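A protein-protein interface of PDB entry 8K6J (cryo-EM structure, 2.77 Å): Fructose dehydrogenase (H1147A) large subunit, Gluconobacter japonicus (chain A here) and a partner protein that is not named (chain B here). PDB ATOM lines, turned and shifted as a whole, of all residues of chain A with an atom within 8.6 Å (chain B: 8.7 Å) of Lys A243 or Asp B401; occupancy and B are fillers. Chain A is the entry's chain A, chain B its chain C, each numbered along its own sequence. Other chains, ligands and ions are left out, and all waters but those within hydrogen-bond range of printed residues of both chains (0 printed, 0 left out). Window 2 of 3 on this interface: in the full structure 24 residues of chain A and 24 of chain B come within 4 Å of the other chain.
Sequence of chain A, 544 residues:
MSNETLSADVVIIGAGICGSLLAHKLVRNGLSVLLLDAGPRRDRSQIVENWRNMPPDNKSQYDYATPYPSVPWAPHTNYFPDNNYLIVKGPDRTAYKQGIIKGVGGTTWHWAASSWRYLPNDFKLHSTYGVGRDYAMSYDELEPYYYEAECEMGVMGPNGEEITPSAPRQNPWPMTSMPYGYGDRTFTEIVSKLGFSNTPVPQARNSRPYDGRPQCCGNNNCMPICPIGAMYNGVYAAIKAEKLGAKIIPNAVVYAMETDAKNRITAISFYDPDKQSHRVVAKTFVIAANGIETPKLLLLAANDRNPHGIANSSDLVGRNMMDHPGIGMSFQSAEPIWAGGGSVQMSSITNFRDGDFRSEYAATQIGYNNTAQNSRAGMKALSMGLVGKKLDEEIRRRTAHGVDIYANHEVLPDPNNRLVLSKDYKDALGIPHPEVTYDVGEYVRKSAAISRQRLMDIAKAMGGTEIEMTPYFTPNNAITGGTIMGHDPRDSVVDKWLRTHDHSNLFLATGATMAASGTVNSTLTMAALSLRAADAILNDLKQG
Among the printed residues, merely in contact across the chains: Asp A211 with Leu B403 (3.4 Å), Tyr A236 with Leu B403 (3.1 Å), Ile A239 with Leu B403 (3.7 Å) and Lys A240 with Leu B403 (3.8 Å).
OD1 of Asp A211 is in salt-bridge range of NZ of Lys A240, 2.7 Å away.
The side-chain amino group (NZ) of Lys A243 is in salt-bridge range of the side-chain carboxylate (OD1) of Asp B401, at 2.6 Å.
Lys A243 touches just one residue of chain B: Asp B401 (2.6 Å). No residue of chain A comes within 4 Å of Pro B400. Of the printed residues of chain B, Lys A240 touches Leu B403. Of the printed residues of chain B, Tyr A236 touches Leu B403. Printed residues of chain A within 4 Å of Leu B403: Asp A211 (3.4 Å), Tyr A236 (3.1 Å), Ile A239 (3.7 Å) and Lys A240 (3.8 Å). Of the printed residues of chain B, Asp A211 touches Leu B403 (3.4 Å). Of the printed residues of chain B, Ile A239 touches Leu B403. Pro B406 touches none of the printed residues of chain A. The nearest residue of chain B that does not touch Lys A243 is Pro B400 (6.1 Å). The nearest printed residue of chain B that does not touch Lys A240 is Ser B402 (7.3 Å).
Of the 17 printed residues of chain A, 5 touch a printed residue of chain B. Hydrophobic or aromatic side chains of chain A that line the printed part of chain B: Tyr A236 and Ile A239. Printed residues of chain B that touch a printed residue of chain A: Asp B401 and Leu B403. Hydrophobic or aromatic side chains of chain B that line the printed part of chain A: Leu B403. Among the printed residues, 5 pairs touch across the chains.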
ATOM      1  N   HIS A  24     -28.661  21.435 -27.024  1.00  0.00           N
ATOM      2  CA  HIS A  24     -27.766  21.598 -25.887  1.00  0.00           C
ATOM      3  C   HIS A  24     -28.349  20.962 -24.636  1.00  0.00           C
ATOM      4  O   HIS A  24     -27.648  20.249 -23.908  1.00  0.00           O
ATOM      5  CB  HIS A  24     -27.487  23.082 -25.658  1.00  0.00           C
ATOM      6  CG  HIS A  24     -26.539  23.353 -24.535  1.00  0.00           C
ATOM      7  ND1 HIS A  24     -26.577  24.514 -23.794  1.00  0.00           N
ATOM      8  CD2 HIS A  24     -25.524  22.616 -24.027  1.00  0.00           C
ATOM      9  CE1 HIS A  24     -25.628  24.479 -22.877  1.00  0.00           C
ATOM     10  NE2 HIS A  24     -24.975  23.339 -22.996  1.00  0.00           N
ATOM     11  N   VAL A  27     -28.130  17.004 -25.122  1.00  0.00           N
ATOM     12  CA  VAL A  27     -26.793  16.443 -24.972  1.00  0.00           C
ATOM     13  C   VAL A  27     -26.246  16.671 -23.573  1.00  0.00           C
ATOM     14  O   VAL A  27     -25.356  15.936 -23.133  1.00  0.00           O
ATOM     15  CB  VAL A  27     -25.825  17.009 -26.025  1.00  0.00           C
ATOM     16  CG1 VAL A  27     -26.348  16.737 -27.414  1.00  0.00           C
ATOM     17  CG2 VAL A  27     -25.609  18.489 -25.810  1.00  0.00           C
ATOM     18  N   ASP A 211     -20.985  34.603 -19.302  1.00  0.00           N
ATOM     19  CA  ASP A 211     -20.890  33.416 -20.152  1.00  0.00           C
ATOM     20  C   ASP A 211     -19.649  33.473 -21.042  1.00  0.00           C
ATOM     21  O   ASP A 211     -19.607  32.881 -22.121  1.00  0.00           O
ATOM     22  CB  ASP A 211     -22.169  33.249 -20.983  1.00  0.00           C
ATOM     23  CG  ASP A 211     -22.199  31.959 -21.775  1.00  0.00           C
ATOM     24  OD1 ASP A 211     -21.783  30.916 -21.229  1.00  0.00           O
ATOM     25  OD2 ASP A 211     -22.640  31.989 -22.942  1.00  0.00           O
ATOM     26  N   GLY A 212     -18.619  34.182 -20.592  1.00  0.00           N
ATOM     27  CA  GLY A 212     -17.442  34.356 -21.414  1.00  0.00           C
ATOM     28  C   GLY A 212     -17.621  35.305 -22.573  1.00  0.00           C
ATOM     29  O   GLY A 212     -16.854  35.242 -23.535  1.00  0.00           O
ATOM     30  N   TYR A 236     -24.430  30.407 -30.264  1.00  0.00           N
ATOM     31  CA  TYR A 236     -23.803  30.054 -28.993  1.00  0.00           C
ATOM     32  C   TYR A 236     -24.293  28.700 -28.502  1.00  0.00           C
ATOM     33  O   TYR A 236     -23.497  27.845 -28.098  1.00  0.00           O
ATOM     34  CB  TYR A 236     -24.080  31.126 -27.942  1.00  0.00           C
ATOM     35  CG  TYR A 236     -23.616  32.507 -28.322  1.00  0.00           C
ATOM     36  CD1 TYR A 236     -22.516  32.690 -29.142  1.00  0.00           C
ATOM     37  CD2 TYR A 236     -24.272  33.628 -27.850  1.00  0.00           C
ATOM     38  CE1 TYR A 236     -22.092  33.949 -29.487  1.00  0.00           C
ATOM     39  CE2 TYR A 236     -23.856  34.889 -28.190  1.00  0.00           C
ATOM     40  CZ  TYR A 236     -22.764  35.045 -29.007  1.00  0.00           C
ATOM     41  OH  TYR A 236     -22.344  36.306 -29.349  1.00  0.00           O
ATOM     42  N   ALA A 237     -25.609  28.487 -28.530  1.00  0.00           N
ATOM     43  CA  ALA A 237     -26.151  27.202 -28.111  1.00  0.00           C
ATOM     44  C   ALA A 237     -25.720  26.092 -29.056  1.00  0.00           C
ATOM     45  O   ALA A 237     -25.450  24.969 -28.620  1.00  0.00           O
ATOM     46  CB  ALA A 237     -27.672  27.273 -28.022  1.00  0.00           C
ATOM     47  N   ALA A 238     -25.648  26.385 -30.357  1.00  0.00           N
ATOM     48  CA  ALA A 238     -25.179  25.378 -31.304  1.00  0.00           C
ATOM     49  C   ALA A 238     -23.738  24.976 -31.012  1.00  0.00           C
ATOM     50  O   ALA A 238     -23.400  23.787 -31.032  1.00  0.00           O
ATOM     51  CB  ALA A 238     -25.314  25.897 -32.734  1.00  0.00           C
ATOM     52  N   ILE A 239     -22.878  25.955 -30.727  1.00  0.00           N
ATOM     53  CA  ILE A 239     -21.482  25.672 -30.413  1.00  0.00           C
ATOM     54  C   ILE A 239     -21.378  24.872 -29.123  1.00  0.00           C
ATOM     55  O   ILE A 239     -20.605  23.911 -29.031  1.00  0.00           O
ATOM     56  CB  ILE A 239     -20.682  26.985 -30.332  1.00  0.00           C
ATOM     57  CG1 ILE A 239     -20.469  27.564 -31.729  1.00  0.00           C
ATOM     58  CG2 ILE A 239     -19.352  26.758 -29.644  1.00  0.00           C
ATOM     59  CD1 ILE A 239     -20.190  29.046 -31.736  1.00  0.00           C
ATOM     60  N   LYS A 240     -22.152  25.254 -28.106  1.00  0.00           N
ATOM     61  CA  LYS A 240     -22.115  24.527 -26.842  1.00  0.00           C
ATOM     62  C   LYS A 240     -22.580  23.087 -27.018  1.00  0.00           C
ATOM     63  O   LYS A 240     -21.996  22.164 -26.442  1.00  0.00           O
ATOM     64  CB  LYS A 240     -22.967  25.245 -25.798  1.00  0.00           C
ATOM     65  CG  LYS A 240     -22.377  26.554 -25.320  1.00  0.00           C
ATOM     66  CD  LYS A 240     -23.205  27.151 -24.202  1.00  0.00           C
ATOM     67  CE  LYS A 240     -22.756  28.561 -23.881  1.00  0.00           C
ATOM     68  NZ  LYS A 240     -23.072  28.928 -22.476  1.00  0.00           N
ATOM     69  N   ALA A 241     -23.636  22.876 -27.807  1.00  0.00           N
ATOM     70  CA  ALA A 241     -24.110  21.520 -28.061  1.00  0.00           C
ATOM     71  C   ALA A 241     -23.078  20.707 -28.828  1.00  0.00           C
ATOM     72  O   ALA A 241     -22.852  19.533 -28.520  1.00  0.00           O
ATOM     73  CB  ALA A 241     -25.433  21.561 -28.821  1.00  0.00           C
ATOM     74  N   GLU A 242     -22.443  21.314 -29.835  1.00  0.00           N
ATOM     75  CA  GLU A 242     -21.421  20.606 -30.597  1.00  0.00           C
ATOM     76  C   GLU A 242     -20.238  20.234 -29.715  1.00  0.00           C
ATOM     77  O   GLU A 242     -19.648  19.158 -29.875  1.00  0.00           O
ATOM     78  CB  GLU A 242     -20.966  21.462 -31.777  1.00  0.00           C
ATOM     79  CG  GLU A 242     -19.899  20.816 -32.638  1.00  0.00           C
ATOM     80  CD  GLU A 242     -20.006  21.218 -34.093  1.00  0.00           C
ATOM     81  OE1 GLU A 242     -20.183  22.424 -34.366  1.00  0.00           O
ATOM     82  OE2 GLU A 242     -19.910  20.330 -34.965  1.00  0.00           O
ATOM     83  N   LYS A 243     -19.873  21.112 -28.780  1.00  0.00           N
ATOM     84  CA  LYS A 243     -18.780  20.813 -27.862  1.00  0.00           C
ATOM     85  C   LYS A 243     -19.100  19.613 -26.979  1.00  0.00           C
ATOM     86  O   LYS A 243     -18.187  18.908 -26.539  1.00  0.00           O
ATOM     87  CB  LYS A 243     -18.475  22.040 -27.003  1.00  0.00           C
ATOM     88  CG  LYS A 243     -17.225  21.919 -26.155  1.00  0.00           C
ATOM     89  CD  LYS A 243     -15.975  21.990 -27.010  1.00  0.00           C
ATOM     90  CE  LYS A 243     -14.732  21.675 -26.198  1.00  0.00           C
ATOM     91  NZ  LYS A 243     -13.491  21.869 -26.995  1.00  0.00           N
ATOM     92  N   LEU A 244     -20.379  19.362 -26.720  1.00  0.00           N
ATOM     93  CA  LEU A 244     -20.798  18.281 -25.841  1.00  0.00           C
ATOM     94  C   LEU A 244     -21.050  16.971 -26.576  1.00  0.00           C
ATOM     95  O   LEU A 244     -21.429  15.985 -25.937  1.00  0.00           O
ATOM     96  CB  LEU A 244     -22.060  18.687 -25.077  1.00  0.00           C
ATOM     97  CG  LEU A 244     -21.840  19.573 -23.855  1.00  0.00           C
ATOM     98  CD1 LEU A 244     -23.161  20.102 -23.340  1.00  0.00           C
ATOM     99  CD2 LEU A 244     -21.114  18.803 -22.773  1.00  0.00           C
ATOM    100  N   GLY A 245     -20.857  16.934 -27.889  1.00  0.00           N
ATOM    101  CA  GLY A 245     -21.006  15.713 -28.661  1.00  0.00           C
ATOM    102  C   GLY A 245     -22.105  15.733 -29.700  1.00  0.00           C
ATOM    103  O   GLY A 245     -22.203  14.781 -30.487  1.00  0.00           O
ATOM    104  N   ALA A 246     -22.946  16.763 -29.745  1.00  0.00           N
ATOM    105  CA  ALA A 246     -23.964  16.841 -30.780  1.00  0.00           C
ATOM    106  C   ALA A 246     -23.316  17.041 -32.142  1.00  0.00           C
ATOM    107  O   ALA A 246     -22.354  17.800 -32.285  1.00  0.00           O
ATOM    108  CB  ALA A 246     -24.937  17.981 -30.491  1.00  0.00           C
ATOM    109  N   LYS A 247     -23.846  16.354 -33.147  1.00  0.00           N
ATOM    110  CA  LYS A 247     -23.335  16.439 -34.507  1.00  0.00           C
ATOM    111  C   LYS A 247     -24.194  17.406 -35.308  1.00  0.00           C
ATOM    112  O   LYS A 247     -25.423  17.286 -35.322  1.00  0.00           O
ATOM    113  CB  LYS A 247     -23.321  15.063 -35.171  1.00  0.00           C
ATOM    114  CG  LYS A 247     -23.106  15.103 -36.672  1.00  0.00           C
ATOM    115  CD  LYS A 247     -21.976  14.180 -37.092  1.00  0.00           C
ATOM    116  CE  LYS A 247     -21.527  14.474 -38.513  1.00  0.00           C
ATOM    117  NZ  LYS A 247     -20.778  15.756 -38.601  1.00  0.00           N
ATOM    118  N   ILE A 248     -23.548  18.361 -35.968  1.00  0.00           N
ATOM    119  CA  ILE A 248     -24.229  19.392 -36.740  1.00  0.00           C
ATOM    120  C   ILE A 248     -23.872  19.198 -38.205  1.00  0.00           C
ATOM    121  O   ILE A 248     -22.689  19.165 -38.564  1.00  0.00           O
ATOM    122  CB  ILE A 248     -23.849  20.801 -36.265  1.00  0.00           C
ATOM    123  CG1 ILE A 248     -24.307  21.019 -34.824  1.00  0.00           C
ATOM    124  CG2 ILE A 248     -24.455  21.850 -37.177  1.00  0.00           C
ATOM    125  CD1 ILE A 248     -23.867  22.337 -34.244  1.00  0.00           C
ATOM    126  N   LEU B 381      -5.918  33.770 -27.880  1.00  0.00           N
ATOM    127  CA  LEU B 381      -6.517  32.443 -27.782  1.00  0.00           C
ATOM    128  C   LEU B 381      -7.505  32.354 -26.627  1.00  0.00           C
ATOM    129  O   LEU B 381      -8.633  31.879 -26.799  1.00  0.00           O
ATOM    130  CB  LEU B 381      -5.422  31.393 -27.619  1.00  0.00           C
ATOM    131  CG  LEU B 381      -4.772  30.875 -28.896  1.00  0.00           C
ATOM    132  CD1 LEU B 381      -3.476  30.172 -28.566  1.00  0.00           C
ATOM    133  CD2 LEU B 381      -5.721  29.944 -29.606  1.00  0.00           C
ATOM    134  N   TYR B 382      -7.099  32.802 -25.440  1.00  0.00           N
ATOM    135  CA  TYR B 382      -7.889  32.612 -24.234  1.00  0.00           C
ATOM    136  C   TYR B 382      -8.607  33.861 -23.761  1.00  0.00           C
ATOM    137  O   TYR B 382      -9.635  33.742 -23.088  1.00  0.00           O
ATOM    138  CB  TYR B 382      -7.001  32.096 -23.094  1.00  0.00           C
ATOM    139  CG  TYR B 382      -6.225  30.855 -23.449  1.00  0.00           C
ATOM    140  CD1 TYR B 382      -6.874  29.651 -23.666  1.00  0.00           C
ATOM    141  CD2 TYR B 382      -4.847  30.887 -23.572  1.00  0.00           C
ATOM    142  CE1 TYR B 382      -6.173  28.513 -23.991  1.00  0.00           C
ATOM    143  CE2 TYR B 382      -4.136  29.753 -23.899  1.00  0.00           C
ATOM    144  CZ  TYR B 382      -4.804  28.570 -24.107  1.00  0.00           C
ATOM    145  OH  TYR B 382      -4.101  27.435 -24.432  1.00  0.00           O
ATOM    146  N   PRO B 396     -13.366  38.572 -25.047  1.00  0.00           N
ATOM    147  CA  PRO B 396     -13.882  37.282 -25.509  1.00  0.00           C
ATOM    148  C   PRO B 396     -12.746  36.428 -26.047  1.00  0.00           C
ATOM    149  O   PRO B 396     -11.849  36.919 -26.734  1.00  0.00           O
ATOM    150  CB  PRO B 396     -14.871  37.670 -26.611  1.00  0.00           C
ATOM    151  CG  PRO B 396     -14.404  39.002 -27.074  1.00  0.00           C
ATOM    152  CD  PRO B 396     -13.857  39.690 -25.865  1.00  0.00           C
ATOM    153  N   ALA B 397     -12.778  35.142 -25.718  1.00  0.00           N
ATOM    154  CA  ALA B 397     -11.782  34.228 -26.249  1.00  0.00           C
ATOM    155  C   ALA B 397     -11.981  34.052 -27.748  1.00  0.00           C
ATOM    156  O   ALA B 397     -13.099  34.121 -28.259  1.00  0.00           O
ATOM    157  CB  ALA B 397     -11.863  32.876 -25.545  1.00  0.00           C
ATOM    158  N   PHE B 398     -10.874  33.833 -28.461  1.00  0.00           N
ATOM    159  CA  PHE B 398     -10.922  33.660 -29.908  1.00  0.00           C
ATOM    160  C   PHE B 398     -10.241  32.372 -30.353  1.00  0.00           C
ATOM    161  O   PHE B 398      -9.827  32.266 -31.510  1.00  0.00           O
ATOM    162  CB  PHE B 398     -10.298  34.861 -30.620  1.00  0.00           C
ATOM    163  CG  PHE B 398     -11.102  36.118 -30.497  1.00  0.00           C
ATOM    164  CD1 PHE B 398     -12.290  36.267 -31.187  1.00  0.00           C
ATOM    165  CD2 PHE B 398     -10.671  37.155 -29.692  1.00  0.00           C
ATOM    166  CE1 PHE B 398     -13.030  37.424 -31.075  1.00  0.00           C
ATOM    167  CE2 PHE B 398     -11.410  38.313 -29.578  1.00  0.00           C
ATOM    168  CZ  PHE B 398     -12.589  38.447 -30.270  1.00  0.00           C
ATOM    169  N   GLY B 399     -10.118  31.392 -29.466  1.00  0.00           N
ATOM    170  CA  GLY B 399      -9.550  30.117 -29.822  1.00  0.00           C
ATOM    171  C   GLY B 399     -10.585  29.217 -30.462  1.00  0.00           C
ATOM    172  O   GLY B 399     -11.669  29.662 -30.847  1.00  0.00           O
ATOM    173  N   PRO B 400     -10.262  27.932 -30.606  1.00  0.00           N
ATOM    174  CA  PRO B 400     -11.249  26.996 -31.164  1.00  0.00           C
ATOM    175  C   PRO B 400     -12.526  26.910 -30.350  1.00  0.00           C
ATOM    176  O   PRO B 400     -13.604  26.715 -30.924  1.00  0.00           O
ATOM    177  CB  PRO B 400     -10.494  25.659 -31.174  1.00  0.00           C
ATOM    178  CG  PRO B 400      -9.056  26.032 -31.141  1.00  0.00           C
ATOM    179  CD  PRO B 400      -8.977  27.279 -30.324  1.00  0.00           C
ATOM    180  N   ASP B 401     -12.440  27.051 -29.028  1.00  0.00           N
ATOM    181  CA  ASP B 401     -13.599  26.983 -28.153  1.00  0.00           C
ATOM    182  C   ASP B 401     -14.291  28.329 -27.990  1.00  0.00           C
ATOM    183  O   ASP B 401     -15.038  28.520 -27.024  1.00  0.00           O
ATOM    184  CB  ASP B 401     -13.195  26.437 -26.783  1.00  0.00           C
ATOM    185  CG  ASP B 401     -12.485  25.105 -26.873  1.00  0.00           C
ATOM    186  OD1 ASP B 401     -12.863  24.288 -27.738  1.00  0.00           O
ATOM    187  OD2 ASP B 401     -11.549  24.875 -26.079  1.00  0.00           O
ATOM    188  N   SER B 402     -14.055  29.264 -28.902  1.00  0.00           N
ATOM    189  CA  SER B 402     -14.647  30.586 -28.785  1.00  0.00           C
ATOM    190  C   SER B 402     -16.145  30.542 -29.051  1.00  0.00           C
ATOM    191  O   SER B 402     -16.635  29.752 -29.862  1.00  0.00           O
ATOM    192  CB  SER B 402     -13.984  31.554 -29.761  1.00  0.00           C
ATOM    193  OG  SER B 402     -14.430  32.877 -29.532  1.00  0.00           O
ATOM    194  N   LEU B 403     -16.875  31.405 -28.350  1.00  0.00           N
ATOM    195  CA  LEU B 403     -18.294  31.596 -28.610  1.00  0.00           C
ATOM    196  C   LEU B 403     -18.536  32.737 -29.585  1.00  0.00           C
ATOM    197  O   LEU B 403     -19.435  32.655 -30.426  1.00  0.00           O
ATOM    198  CB  LEU B 403     -19.039  31.867 -27.304  1.00  0.00           C
ATOM    199  CG  LEU B 403     -19.401  30.658 -26.445  1.00  0.00           C
ATOM    200  CD1 LEU B 403     -20.363  31.062 -25.347  1.00  0.00           C
ATOM    201  CD2 LEU B 403     -19.995  29.560 -27.300  1.00  0.00           C
ATOM    202  N   VAL B 404     -17.739  33.801 -29.489  1.00  0.00           N
ATOM    203  CA  VAL B 404     -17.939  34.968 -30.340  1.00  0.00           C
ATOM    204  C   VAL B 404     -17.501  34.667 -31.768  1.00  0.00           C
ATOM    205  O   VAL B 404     -18.295  34.747 -32.711  1.00  0.00           O
ATOM    206  CB  VAL B 404     -17.191  36.183 -29.768  1.00  0.00           C
ATOM    207  CG1 VAL B 404     -17.185  37.318 -30.769  1.00  0.00           C
ATOM    208  CG2 VAL B 404     -17.829  36.620 -28.469  1.00  0.00           C
ATOM    209  N   GLN B 405     -16.235  34.313 -31.946  1.00  0.00           N
ATOM    210  CA  GLN B 405     -15.681  34.050 -33.274  1.00  0.00           C
ATOM    211  C   GLN B 405     -14.512  33.091 -33.132  1.00  0.00           C
ATOM    212  O   GLN B 405     -13.397  33.503 -32.779  1.00  0.00           O
ATOM    213  CB  GLN B 405     -15.246  35.340 -33.964  1.00  0.00           C
ATOM    214  CG  GLN B 405     -14.560  35.126 -35.297  1.00  0.00           C
ATOM    215  CD  GLN B 405     -15.314  34.171 -36.190  1.00  0.00           C
ATOM    216  OE1 GLN B 405     -16.381  34.497 -36.704  1.00  0.00           O
ATOM    217  NE2 GLN B 405     -14.765  32.980 -36.379  1.00  0.00           N
ATOM    218  N   PRO B 406     -14.724  31.801 -33.381  1.00  0.00           N
ATOM    219  CA  PRO B 406     -13.595  30.866 -33.402  1.00  0.00           C
ATOM    220  C   PRO B 406     -12.626  31.215 -34.519  1.00  0.00           C
ATOM    221  O   PRO B 406     -13.023  31.660 -35.597  1.00  0.00           O
ATOM    222  CB  PRO B 406     -14.262  29.507 -33.638  1.00  0.00           C
ATOM    223  CG  PRO B 406     -15.693  29.705 -33.270  1.00  0.00           C
ATOM    224  CD  PRO B 406     -16.009  31.122 -33.603  1.00  0.00           C
ATOM    225  N   LEU B 407     -11.340  31.007 -34.255  1.00  0.00           N
ATOM    226  CA  LEU B 407     -10.294  31.302 -35.219  1.00  0.00           C
ATOM    227  C   LEU B 407      -9.354  30.114 -35.340  1.00  0.00           C
ATOM    228  O   LEU B 407      -9.119  29.386 -34.372  1.00  0.00           O
ATOM    229  CB  LEU B 407      -9.500  32.551 -34.824  1.00  0.00           C
ATOM    230  CG  LEU B 407     -10.230  33.891 -34.872  1.00  0.00           C
ATOM    231  CD1 LEU B 407      -9.337  34.996 -34.347  1.00  0.00           C
ATOM    232  CD2 LEU B 407     -10.679  34.198 -36.284  1.00  0.00           C
ATOM    233  N   ILE B 412      -5.178  33.215 -36.582  1.00  0.00           N
ATOM    234  CA  ILE B 412      -4.615  33.840 -35.390  1.00  0.00           C
ATOM    235  C   ILE B 412      -3.190  34.298 -35.656  1.00  0.00           C
ATOM    236  O   ILE B 412      -2.782  35.382 -35.226  1.00  0.00           O
ATOM    237  CB  ILE B 412      -4.690  32.874 -34.194  1.00  0.00           C
ATOM    238  CG1 ILE B 412      -6.123  32.793 -33.678  1.00  0.00           C
ATOM    239  CG2 ILE B 412      -3.767  33.322 -33.082  1.00  0.00           C
ATOM    240  CD1 ILE B 412      -6.322  31.763 -32.610  1.00  0.00           C
ATOM    241  N   ARG B 439      -1.529  26.606 -27.827  1.00  0.00           N
ATOM    242  CA  ARG B 439      -2.769  25.898 -27.530  1.00  0.00           C
ATOM    243  C   ARG B 439      -2.499  24.608 -26.774  1.00  0.00           C
ATOM    244  O   ARG B 439      -3.221  24.270 -25.830  1.00  0.00           O
ATOM    245  CB  ARG B 439      -3.525  25.597 -28.821  1.00  0.00           C
ATOM    246  CG  ARG B 439      -4.516  26.658 -29.227  1.00  0.00           C
ATOM    247  CD  ARG B 439      -5.513  26.115 -30.230  1.00  0.00           C
ATOM    248  NE  ARG B 439      -4.861  25.593 -31.422  1.00  0.00           N
ATOM    249  CZ  ARG B 439      -4.890  24.320 -31.794  1.00  0.00           C
ATOM    250  NH1 ARG B 439      -5.534  23.409 -31.085  1.00  0.00           N
ATOM    251  NH2 ARG B 439      -4.256  23.955 -32.903  1.00  0.00           N
